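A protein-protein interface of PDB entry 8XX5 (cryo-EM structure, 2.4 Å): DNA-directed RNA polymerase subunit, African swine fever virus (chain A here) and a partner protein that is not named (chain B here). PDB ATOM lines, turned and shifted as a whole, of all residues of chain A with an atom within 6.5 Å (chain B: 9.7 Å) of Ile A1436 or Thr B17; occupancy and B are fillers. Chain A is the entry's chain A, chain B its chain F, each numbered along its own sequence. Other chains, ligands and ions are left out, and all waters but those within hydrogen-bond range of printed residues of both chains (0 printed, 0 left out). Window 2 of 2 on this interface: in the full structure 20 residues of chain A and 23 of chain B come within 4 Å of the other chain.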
ATOM      1  N   MET A1431      22.368  11.846   5.428  1.00  0.00           N
ATOM      2  CA  MET A1431      23.684  11.228   5.428  1.00  0.00           C
ATOM      3  C   MET A1431      24.538  11.831   4.319  1.00  0.00           C
ATOM      4  O   MET A1431      24.074  11.988   3.186  1.00  0.00           O
ATOM      5  CB  MET A1431      23.570   9.714   5.246  1.00  0.00           C
ATOM      6  CG  MET A1431      22.538   9.060   6.145  1.00  0.00           C
ATOM      7  SD  MET A1431      23.050   8.922   7.866  1.00  0.00           S
ATOM      8  CE  MET A1431      24.731   8.340   7.700  1.00  0.00           C
ATOM      9  N   ASP A1432      25.781  12.172   4.651  1.00  0.00           N
ATOM     10  CA  ASP A1432      26.738  12.693   3.675  1.00  0.00           C
ATOM     11  C   ASP A1432      27.267  11.518   2.865  1.00  0.00           C
ATOM     12  O   ASP A1432      28.300  10.932   3.183  1.00  0.00           O
ATOM     13  CB  ASP A1432      27.869  13.442   4.366  1.00  0.00           C
ATOM     14  CG  ASP A1432      28.658  14.317   3.411  1.00  0.00           C
ATOM     15  OD1 ASP A1432      28.425  14.233   2.188  1.00  0.00           O
ATOM     16  OD2 ASP A1432      29.518  15.088   3.884  1.00  0.00           O
ATOM     17  N   GLU A1433      26.551  11.185   1.788  1.00  0.00           N
ATOM     18  CA  GLU A1433      26.866   9.978   1.030  1.00  0.00           C
ATOM     19  C   GLU A1433      28.277  10.024   0.459  1.00  0.00           C
ATOM     20  O   GLU A1433      29.013   9.035   0.534  1.00  0.00           O
ATOM     21  CB  GLU A1433      25.841   9.779  -0.084  1.00  0.00           C
ATOM     22  CG  GLU A1433      24.638   8.955   0.335  1.00  0.00           C
ATOM     23  CD  GLU A1433      23.332   9.520  -0.186  1.00  0.00           C
ATOM     24  OE1 GLU A1433      23.365  10.561  -0.875  1.00  0.00           O
ATOM     25  OE2 GLU A1433      22.273   8.921   0.094  1.00  0.00           O
ATOM     26  N   LYS A1434      28.675  11.163  -0.109  1.00  0.00           N
ATOM     27  CA  LYS A1434      30.024  11.287  -0.655  1.00  0.00           C
ATOM     28  C   LYS A1434      31.074  11.023   0.416  1.00  0.00           C
ATOM     29  O   LYS A1434      32.003  10.230   0.213  1.00  0.00           O
ATOM     30  CB  LYS A1434      30.212  12.678  -1.260  1.00  0.00           C
ATOM     31  CG  LYS A1434      31.120  12.717  -2.476  1.00  0.00           C
ATOM     32  CD  LYS A1434      31.393  14.148  -2.916  1.00  0.00           C
ATOM     33  CE  LYS A1434      31.563  15.077  -1.723  1.00  0.00           C
ATOM     34  NZ  LYS A1434      32.246  16.348  -2.090  1.00  0.00           N
ATOM     35  N   TYR A1435      30.927  11.667   1.575  1.00  0.00           N
ATOM     36  CA  TYR A1435      31.894  11.504   2.653  1.00  0.00           C
ATOM     37  C   TYR A1435      31.916  10.076   3.182  1.00  0.00           C
ATOM     38  O   TYR A1435      32.984   9.558   3.521  1.00  0.00           O
ATOM     39  CB  TYR A1435      31.580  12.485   3.781  1.00  0.00           C
ATOM     40  CG  TYR A1435      32.641  12.560   4.848  1.00  0.00           C
ATOM     41  CD1 TYR A1435      33.778  13.329   4.666  1.00  0.00           C
ATOM     42  CD2 TYR A1435      32.504  11.868   6.042  1.00  0.00           C
ATOM     43  CE1 TYR A1435      34.750  13.404   5.636  1.00  0.00           C
ATOM     44  CE2 TYR A1435      33.470  11.938   7.019  1.00  0.00           C
ATOM     45  CZ  TYR A1435      34.592  12.708   6.810  1.00  0.00           C
ATOM     46  OH  TYR A1435      35.564  12.788   7.777  1.00  0.00           O
ATOM     47  N   ILE A1436      30.754   9.429   3.272  1.00  0.00           N
ATOM     48  CA  ILE A1436      30.713   8.062   3.777  1.00  0.00           C
ATOM     49  C   ILE A1436      31.364   7.102   2.789  1.00  0.00           C
ATOM     50  O   ILE A1436      32.068   6.168   3.188  1.00  0.00           O
ATOM     51  CB  ILE A1436      29.266   7.653   4.106  1.00  0.00           C
ATOM     52  CG1 ILE A1436      28.703   8.525   5.225  1.00  0.00           C
ATOM     53  CG2 ILE A1436      29.210   6.223   4.566  1.00  0.00           C
ATOM     54  CD1 ILE A1436      27.214   8.748   5.127  1.00  0.00           C
ATOM     55  N   THR A1437      31.145   7.309   1.488  1.00  0.00           N
ATOM     56  CA  THR A1437      31.806   6.474   0.488  1.00  0.00           C
ATOM     57  C   THR A1437      33.317   6.671   0.514  1.00  0.00           C
ATOM     58  O   THR A1437      34.082   5.709   0.393  1.00  0.00           O
ATOM     59  CB  THR A1437      31.259   6.770  -0.912  1.00  0.00           C
ATOM     60  OG1 THR A1437      31.528   8.134  -1.257  1.00  0.00           O
ATOM     61  CG2 THR A1437      29.769   6.496  -0.991  1.00  0.00           C
ATOM     62  N   GLU A1438      33.771   7.915   0.665  1.00  0.00           N
ATOM     63  CA  GLU A1438      35.202   8.167   0.549  1.00  0.00           C
ATOM     64  C   GLU A1438      35.925   8.078   1.889  1.00  0.00           C
ATOM     65  O   GLU A1438      37.139   8.294   1.948  1.00  0.00           O
ATOM     66  CB  GLU A1438      35.453   9.529  -0.105  1.00  0.00           C
ATOM     67  CG  GLU A1438      35.012  10.716   0.720  1.00  0.00           C
ATOM     68  CD  GLU A1438      35.238  12.037   0.016  1.00  0.00           C
ATOM     69  OE1 GLU A1438      34.953  12.124  -1.195  1.00  0.00           O
ATOM     70  OE2 GLU A1438      35.699  12.989   0.679  1.00  0.00           O
ATOM     71  N   ASN A1439      35.208   7.761   2.969  1.00  0.00           N
ATOM     72  CA  ASN A1439      35.867   7.560   4.258  1.00  0.00           C
ATOM     73  C   ASN A1439      35.306   6.380   5.043  1.00  0.00           C
ATOM     74  O   ASN A1439      35.518   6.311   6.258  1.00  0.00           O
ATOM     75  CB  ASN A1439      35.769   8.814   5.137  1.00  0.00           C
ATOM     76  CG  ASN A1439      36.289  10.061   4.456  1.00  0.00           C
ATOM     77  OD1 ASN A1439      35.570  10.723   3.715  1.00  0.00           O
ATOM     78  ND2 ASN A1439      37.548  10.391   4.712  1.00  0.00           N
ATOM     79  N   TYR A1440      34.625   5.452   4.366  1.00  0.00           N
ATOM     80  CA  TYR A1440      33.932   4.298   4.978  1.00  0.00           C
ATOM     81  C   TYR A1440      33.800   4.306   6.499  1.00  0.00           C
ATOM     82  O   TYR A1440      34.672   3.798   7.205  1.00  0.00           O
ATOM     83  CB  TYR A1440      34.613   2.987   4.571  1.00  0.00           C
ATOM     84  CG  TYR A1440      34.219   2.470   3.205  1.00  0.00           C
ATOM     85  CD1 TYR A1440      33.638   3.306   2.263  1.00  0.00           C
ATOM     86  CD2 TYR A1440      34.399   1.135   2.873  1.00  0.00           C
ATOM     87  CE1 TYR A1440      33.273   2.831   1.018  1.00  0.00           C
ATOM     88  CE2 TYR A1440      34.032   0.650   1.632  1.00  0.00           C
ATOM     89  CZ  TYR A1440      33.467   1.503   0.709  1.00  0.00           C
ATOM     90  OH  TYR A1440      33.099   1.027  -0.529  1.00  0.00           O
ATOM     91  N   ILE B  13      15.610   2.264   6.076  1.00  0.00           N
ATOM     92  CA  ILE B  13      17.027   1.945   6.160  1.00  0.00           C
ATOM     93  C   ILE B  13      17.387   1.793   7.630  1.00  0.00           C
ATOM     94  O   ILE B  13      17.434   2.779   8.373  1.00  0.00           O
ATOM     95  CB  ILE B  13      17.885   3.021   5.486  1.00  0.00           C
ATOM     96  CG1 ILE B  13      17.560   3.098   3.994  1.00  0.00           C
ATOM     97  CG2 ILE B  13      19.333   2.714   5.691  1.00  0.00           C
ATOM     98  CD1 ILE B  13      17.590   4.492   3.442  1.00  0.00           C
ATOM     99  N   ASP B  14      17.652   0.555   8.051  1.00  0.00           N
ATOM    100  CA  ASP B  14      17.976   0.290   9.446  1.00  0.00           C
ATOM    101  C   ASP B  14      19.427   0.594   9.789  1.00  0.00           C
ATOM    102  O   ASP B  14      19.753   0.726  10.973  1.00  0.00           O
ATOM    103  CB  ASP B  14      17.660  -1.164   9.791  1.00  0.00           C
ATOM    104  CG  ASP B  14      16.171  -1.439   9.836  1.00  0.00           C
ATOM    105  OD1 ASP B  14      15.448  -0.949   8.944  1.00  0.00           O
ATOM    106  OD2 ASP B  14      15.724  -2.143  10.765  1.00  0.00           O
ATOM    107  N   ASP B  15      20.302   0.701   8.793  1.00  0.00           N
ATOM    108  CA  ASP B  15      21.707   1.049   9.009  1.00  0.00           C
ATOM    109  C   ASP B  15      22.109   2.100   7.986  1.00  0.00           C
ATOM    110  O   ASP B  15      22.767   1.798   6.984  1.00  0.00           O
ATOM    111  CB  ASP B  15      22.603  -0.188   8.916  1.00  0.00           C
ATOM    112  CG  ASP B  15      23.872  -0.049   9.728  1.00  0.00           C
ATOM    113  OD1 ASP B  15      24.512   1.021   9.653  1.00  0.00           O
ATOM    114  OD2 ASP B  15      24.233  -1.008  10.442  1.00  0.00           O
ATOM    115  N   PRO B  16      21.714   3.358   8.205  1.00  0.00           N
ATOM    116  CA  PRO B  16      21.977   4.394   7.190  1.00  0.00           C
ATOM    117  C   PRO B  16      23.447   4.592   6.867  1.00  0.00           C
ATOM    118  O   PRO B  16      23.780   4.855   5.705  1.00  0.00           O
ATOM    119  CB  PRO B  16      21.358   5.656   7.809  1.00  0.00           C
ATOM    120  CG  PRO B  16      21.216   5.357   9.259  1.00  0.00           C
ATOM    121  CD  PRO B  16      20.986   3.889   9.366  1.00  0.00           C
ATOM    122  N   THR B  17      24.338   4.480   7.851  1.00  0.00           N
ATOM    123  CA  THR B  17      25.760   4.646   7.567  1.00  0.00           C
ATOM    124  C   THR B  17      26.304   3.477   6.753  1.00  0.00           C
ATOM    125  O   THR B  17      27.136   3.670   5.860  1.00  0.00           O
ATOM    126  CB  THR B  17      26.542   4.821   8.870  1.00  0.00           C
ATOM    127  OG1 THR B  17      27.942   4.640   8.622  1.00  0.00           O
ATOM    128  CG2 THR B  17      26.072   3.832   9.921  1.00  0.00           C
ATOM    129  N   ASN B  18      25.848   2.259   7.045  1.00  0.00           N
ATOM    130  CA  ASN B  18      26.250   1.102   6.254  1.00  0.00           C
ATOM    131  C   ASN B  18      25.521   1.041   4.920  1.00  0.00           C
ATOM    132  O   ASN B  18      26.087   0.558   3.935  1.00  0.00           O
ATOM    133  CB  ASN B  18      26.007  -0.186   7.038  1.00  0.00           C
ATOM    134  CG  ASN B  18      25.917  -1.402   6.142  1.00  0.00           C
ATOM    135  OD1 ASN B  18      26.892  -1.779   5.493  1.00  0.00           O
ATOM    136  ND2 ASN B  18      24.742  -2.015   6.091  1.00  0.00           N
ATOM    137  N   PHE B  19      24.269   1.504   4.870  1.00  0.00           N
ATOM    138  CA  PHE B  19      23.542   1.544   3.604  1.00  0.00           C
ATOM    139  C   PHE B  19      24.242   2.435   2.593  1.00  0.00           C
ATOM    140  O   PHE B  19      24.136   2.208   1.383  1.00  0.00           O
ATOM    141  CB  PHE B  19      22.114   2.028   3.839  1.00  0.00           C
ATOM    142  CG  PHE B  19      21.301   2.169   2.585  1.00  0.00           C
ATOM    143  CD1 PHE B  19      20.623   1.085   2.060  1.00  0.00           C
ATOM    144  CD2 PHE B  19      21.195   3.392   1.945  1.00  0.00           C
ATOM    145  CE1 PHE B  19      19.869   1.213   0.916  1.00  0.00           C
ATOM    146  CE2 PHE B  19      20.445   3.525   0.798  1.00  0.00           C
ATOM    147  CZ  PHE B  19      19.780   2.434   0.283  1.00  0.00           C
ATOM    148  N   CYS B  20      24.962   3.445   3.064  1.00  0.00           N
ATOM    149  CA  CYS B  20      25.826   4.231   2.199  1.00  0.00           C
ATOM    150  C   CYS B  20      27.082   3.411   1.905  1.00  0.00           C
ATOM    151  O   CYS B  20      27.137   2.206   2.164  1.00  0.00           O
ATOM    152  CB  CYS B  20      26.129   5.582   2.837  1.00  0.00           C
ATOM    153  SG  CYS B  20      24.666   6.598   3.145  1.00  0.00           S
ATOM    154  N   THR B  21      28.086   4.055   1.310  1.00  0.00           N
ATOM    155  CA  THR B  21      29.305   3.441   0.782  1.00  0.00           C
ATOM    156  C   THR B  21      28.983   2.641  -0.475  1.00  0.00           C
ATOM    157  O   THR B  21      29.882   2.282  -1.242  1.00  0.00           O
ATOM    158  CB  THR B  21      29.995   2.525   1.806  1.00  0.00           C
ATOM    159  OG1 THR B  21      29.216   1.336   1.992  1.00  0.00           O
ATOM    160  CG2 THR B  21      30.178   3.217   3.139  1.00  0.00           C
ATOM    161  N   ASN B  22      27.696   2.369  -0.689  1.00  0.00           N
ATOM    162  CA  ASN B  22      27.187   1.914  -1.979  1.00  0.00           C
ATOM    163  C   ASN B  22      25.681   2.154  -1.927  1.00  0.00           C
ATOM    164  O   ASN B  22      24.951   1.352  -1.340  1.00  0.00           O
ATOM    165  CB  ASN B  22      27.517   0.452  -2.232  1.00  0.00           C
ATOM    166  CG  ASN B  22      27.599   0.126  -3.704  1.00  0.00           C
ATOM    167  OD1 ASN B  22      27.172   0.912  -4.550  1.00  0.00           O
ATOM    168  ND2 ASN B  22      28.151  -1.038  -4.022  1.00  0.00           N
ATOM    169  N   VAL B  23      25.224   3.243  -2.533  1.00  0.00           N
ATOM    170  CA  VAL B  23      23.813   3.584  -2.411  1.00  0.00           C
ATOM    171  C   VAL B  23      22.994   2.973  -3.538  1.00  0.00           C
ATOM    172  O   VAL B  23      21.920   2.421  -3.296  1.00  0.00           O
ATOM    173  CB  VAL B  23      23.630   5.110  -2.346  1.00  0.00           C
ATOM    174  CG1 VAL B  23      22.160   5.454  -2.416  1.00  0.00           C
ATOM    175  CG2 VAL B  23      24.239   5.653  -1.069  1.00  0.00           C
ATOM    176  N   HIS B  26      22.845  -1.022  -2.987  1.00  0.00           N
ATOM    177  CA  HIS B  26      21.990  -1.376  -1.859  1.00  0.00           C
ATOM    178  C   HIS B  26      20.535  -1.030  -2.145  1.00  0.00           C
ATOM    179  O   HIS B  26      19.624  -1.775  -1.766  1.00  0.00           O
ATOM    180  CB  HIS B  26      22.472  -0.669  -0.595  1.00  0.00           C
ATOM    181  CG  HIS B  26      23.826  -1.109  -0.135  1.00  0.00           C
ATOM    182  ND1 HIS B  26      24.635  -0.321   0.654  1.00  0.00           N
ATOM    183  CD2 HIS B  26      24.512  -2.256  -0.348  1.00  0.00           C
ATOM    184  CE1 HIS B  26      25.762  -0.962   0.904  1.00  0.00           C
ATOM    185  NE2 HIS B  26      25.712  -2.139   0.308  1.00  0.00           N
ATOM    186  N   ARG B  54      15.931   9.571  -6.765  1.00  0.00           N
ATOM    187  CA  ARG B  54      15.940   9.144  -5.378  1.00  0.00           C
ATOM    188  C   ARG B  54      16.149  10.360  -4.492  1.00  0.00           C
ATOM    189  O   ARG B  54      16.588  11.417  -4.946  1.00  0.00           O
ATOM    190  CB  ARG B  54      17.023   8.092  -5.123  1.00  0.00           C
ATOM    191  CG  ARG B  54      18.366   8.692  -4.790  1.00  0.00           C
ATOM    192  CD  ARG B  54      19.272   7.705  -4.094  1.00  0.00           C
ATOM    193  NE  ARG B  54      20.669   8.051  -4.310  1.00  0.00           N
ATOM    194  CZ  ARG B  54      21.469   8.531  -3.369  1.00  0.00           C
ATOM    195  NH1 ARG B  54      21.039   8.742  -2.138  1.00  0.00           N
ATOM    196  NH2 ARG B  54      22.734   8.808  -3.673  1.00  0.00           N
ATOM    197  N   CYS B  57      19.214  10.273   2.001  1.00  0.00           N
ATOM    198  CA  CYS B  57      18.865   9.377   3.103  1.00  0.00           C
ATOM    199  C   CYS B  57      18.542  10.223   4.332  1.00  0.00           C
ATOM    200  O   CYS B  57      19.382  10.473   5.200  1.00  0.00           O
ATOM    201  CB  CYS B  57      19.992   8.391   3.377  1.00  0.00           C
ATOM    202  SG  CYS B  57      19.630   7.191   4.678  1.00  0.00           S
ATOM    203  N   PHE B  58      17.294  10.678   4.396  1.00  0.00           N
ATOM    204  CA  PHE B  58      16.836  11.433   5.552  1.00  0.00           C
ATOM    205  C   PHE B  58      16.789  10.535   6.780  1.00  0.00           C
ATOM    206  O   PHE B  58      16.400   9.371   6.697  1.00  0.00           O
ATOM    207  CB  PHE B  58      15.444  12.013   5.310  1.00  0.00           C
ATOM    208  CG  PHE B  58      15.307  12.773   4.030  1.00  0.00           C
ATOM    209  CD1 PHE B  58      15.827  14.044   3.905  1.00  0.00           C
ATOM    210  CD2 PHE B  58      14.622  12.227   2.962  1.00  0.00           C
ATOM    211  CE1 PHE B  58      15.690  14.746   2.730  1.00  0.00           C
ATOM    212  CE2 PHE B  58      14.481  12.926   1.787  1.00  0.00           C
ATOM    213  CZ  PHE B  58      15.015  14.187   1.669  1.00  0.00           C
ATOM    214  N   ILE B  59      17.170  11.086   7.923  1.00  0.00           N
ATOM    215  CA  ILE B  59      17.074  10.367   9.186  1.00  0.00           C
ATOM    216  C   ILE B  59      15.656  10.495   9.720  1.00  0.00           C
ATOM    217  O   ILE B  59      15.041  11.564   9.633  1.00  0.00           O
ATOM    218  CB  ILE B  59      18.110  10.901  10.191  1.00  0.00           C
ATOM    219  CG1 ILE B  59      19.522  10.706   9.643  1.00  0.00           C
ATOM    220  CG2 ILE B  59      17.972  10.203  11.535  1.00  0.00           C
ATOM    221  CD1 ILE B  59      19.769   9.322   9.102  1.00  0.00           C
ATOM    222  N   GLY B  66      17.265   6.413  14.949  1.00  0.00           N
ATOM    223  CA  GLY B  66      18.397   6.770  14.121  1.00  0.00           C
ATOM    224  C   GLY B  66      18.356   6.214  12.719  1.00  0.00           C
ATOM    225  O   GLY B  66      19.338   6.358  11.983  1.00  0.00           O
ATOM    226  N   ARG B  67      17.256   5.584  12.325  1.00  0.00           N
ATOM    227  CA  ARG B  67      17.145   4.976  11.011  1.00  0.00           C
ATOM    228  C   ARG B  67      16.817   6.026   9.953  1.00  0.00           C
ATOM    229  O   ARG B  67      16.314   7.113  10.248  1.00  0.00           O
ATOM    230  CB  ARG B  67      16.074   3.888  11.019  1.00  0.00           C
ATOM    231  CG  ARG B  67      16.461   2.643  11.788  1.00  0.00           C
ATOM    232  CD  ARG B  67      15.253   2.002  12.441  1.00  0.00           C
ATOM    233  NE  ARG B  67      14.177   1.764  11.488  1.00  0.00           N
ATOM    234  CZ  ARG B  67      12.908   2.090  11.694  1.00  0.00           C
ATOM    235  NH1 ARG B  67      12.518   2.676  12.814  1.00  0.00           N
ATOM    236  NH2 ARG B  67      12.009   1.825  10.751  1.00  0.00           N
ATOM    237  N   GLY B  68      17.118   5.686   8.704  1.00  0.00           N
ATOM    238  CA  GLY B  68      16.785   6.539   7.583  1.00  0.00           C
ATOM    239  C   GLY B  68      15.708   5.921   6.719  1.00  0.00           C
ATOM    240  O   GLY B  68      15.427   4.729   6.864  1.00  0.00           O
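The side-chain carboxylate of Glu A1433 lies within salt-bridge range of the guanidinium group of Arg B54. N of Met A1431 is in hydrogen-bond range of O of Cys B57.
The backbone carbonyl oxygen (O) of Pro B16 is in hydrogen-bond range of the side-chain sulfur (SG) of Cys B20, 3.2 Å away. The backbone carbonyl oxygen of Glu A1433 sits close to the side-chain hydroxyl of Thr A1437 (3.2 Å). O of Lys A1434 is in hydrogen-bond range of OG1 of Thr A1437 (2.6 Å).
Met A1431 touches Pro B16 (SD to CB, 3.7 Å). Met A1431 touches Ile B59 (SD to CD1, 3.5 Å). Cys B20 touches Glu A1433. CG of Glu A1433 touches CG2 of Val B23, at 3.6 Å. OE2 of Glu A1433 touches N of Cys B57 (3.8 Å). CG2 of Ile A1436 touches O of Thr B17, 3.5 Å away. Ile A1436 touches Cys B20 (CG2 to CB, 3.6 Å). Ile A1436 touches Thr B21. Thr A1437 touches Thr B21. Tyr A1440 touches Thr B21 (CE1 to CB, 3.4 Å).
Printed residues of chain B within 4 Å of Met A1431: Pro B16 (3.7 Å), Thr B17 (3.8 Å), Cys B20 (3.9 Å), Cys B57 (3.3 Å) and Ile B59 (3.5 Å). Of the printed residues of chain B, Glu A1433 touches Cys B20, Val B23, Arg B54 and Cys B57. Of chain B, only Thr B17 (3.5 Å), Cys B20 (3.6 Å) and Thr B21 (3.5 Å) come within 4 Å of Ile A1436. Printed residues of chain B within 4 Å of Thr A1437: Thr B21. Of chain A, only Met A1431 and Ile A1436 come within 4 Å of Thr B17. Asn B18 touches none of the printed residues of chain A. Of the printed residues of chain A, Cys B20 touches Met A1431, Glu A1433 and Ile A1436. Of the printed residues of chain A, Val B23 touches Glu A1433 (3.6 Å). Of the printed residues of chain A, Arg B54 touches Glu A1433. Gly B66 touches none of the printed residues of chain A. The nearest residue of chain A that does not touch Thr B17 is Tyr A1440 (6.2 Å).
Among the printed residues, 14 pairs touch across the chains. Among the printed residues, Asp or Glu carboxylates within 4 Å of a Lys or Arg side-chain nitrogen of the other chain: Glu A1433 with Arg B54 (2.6 Å).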
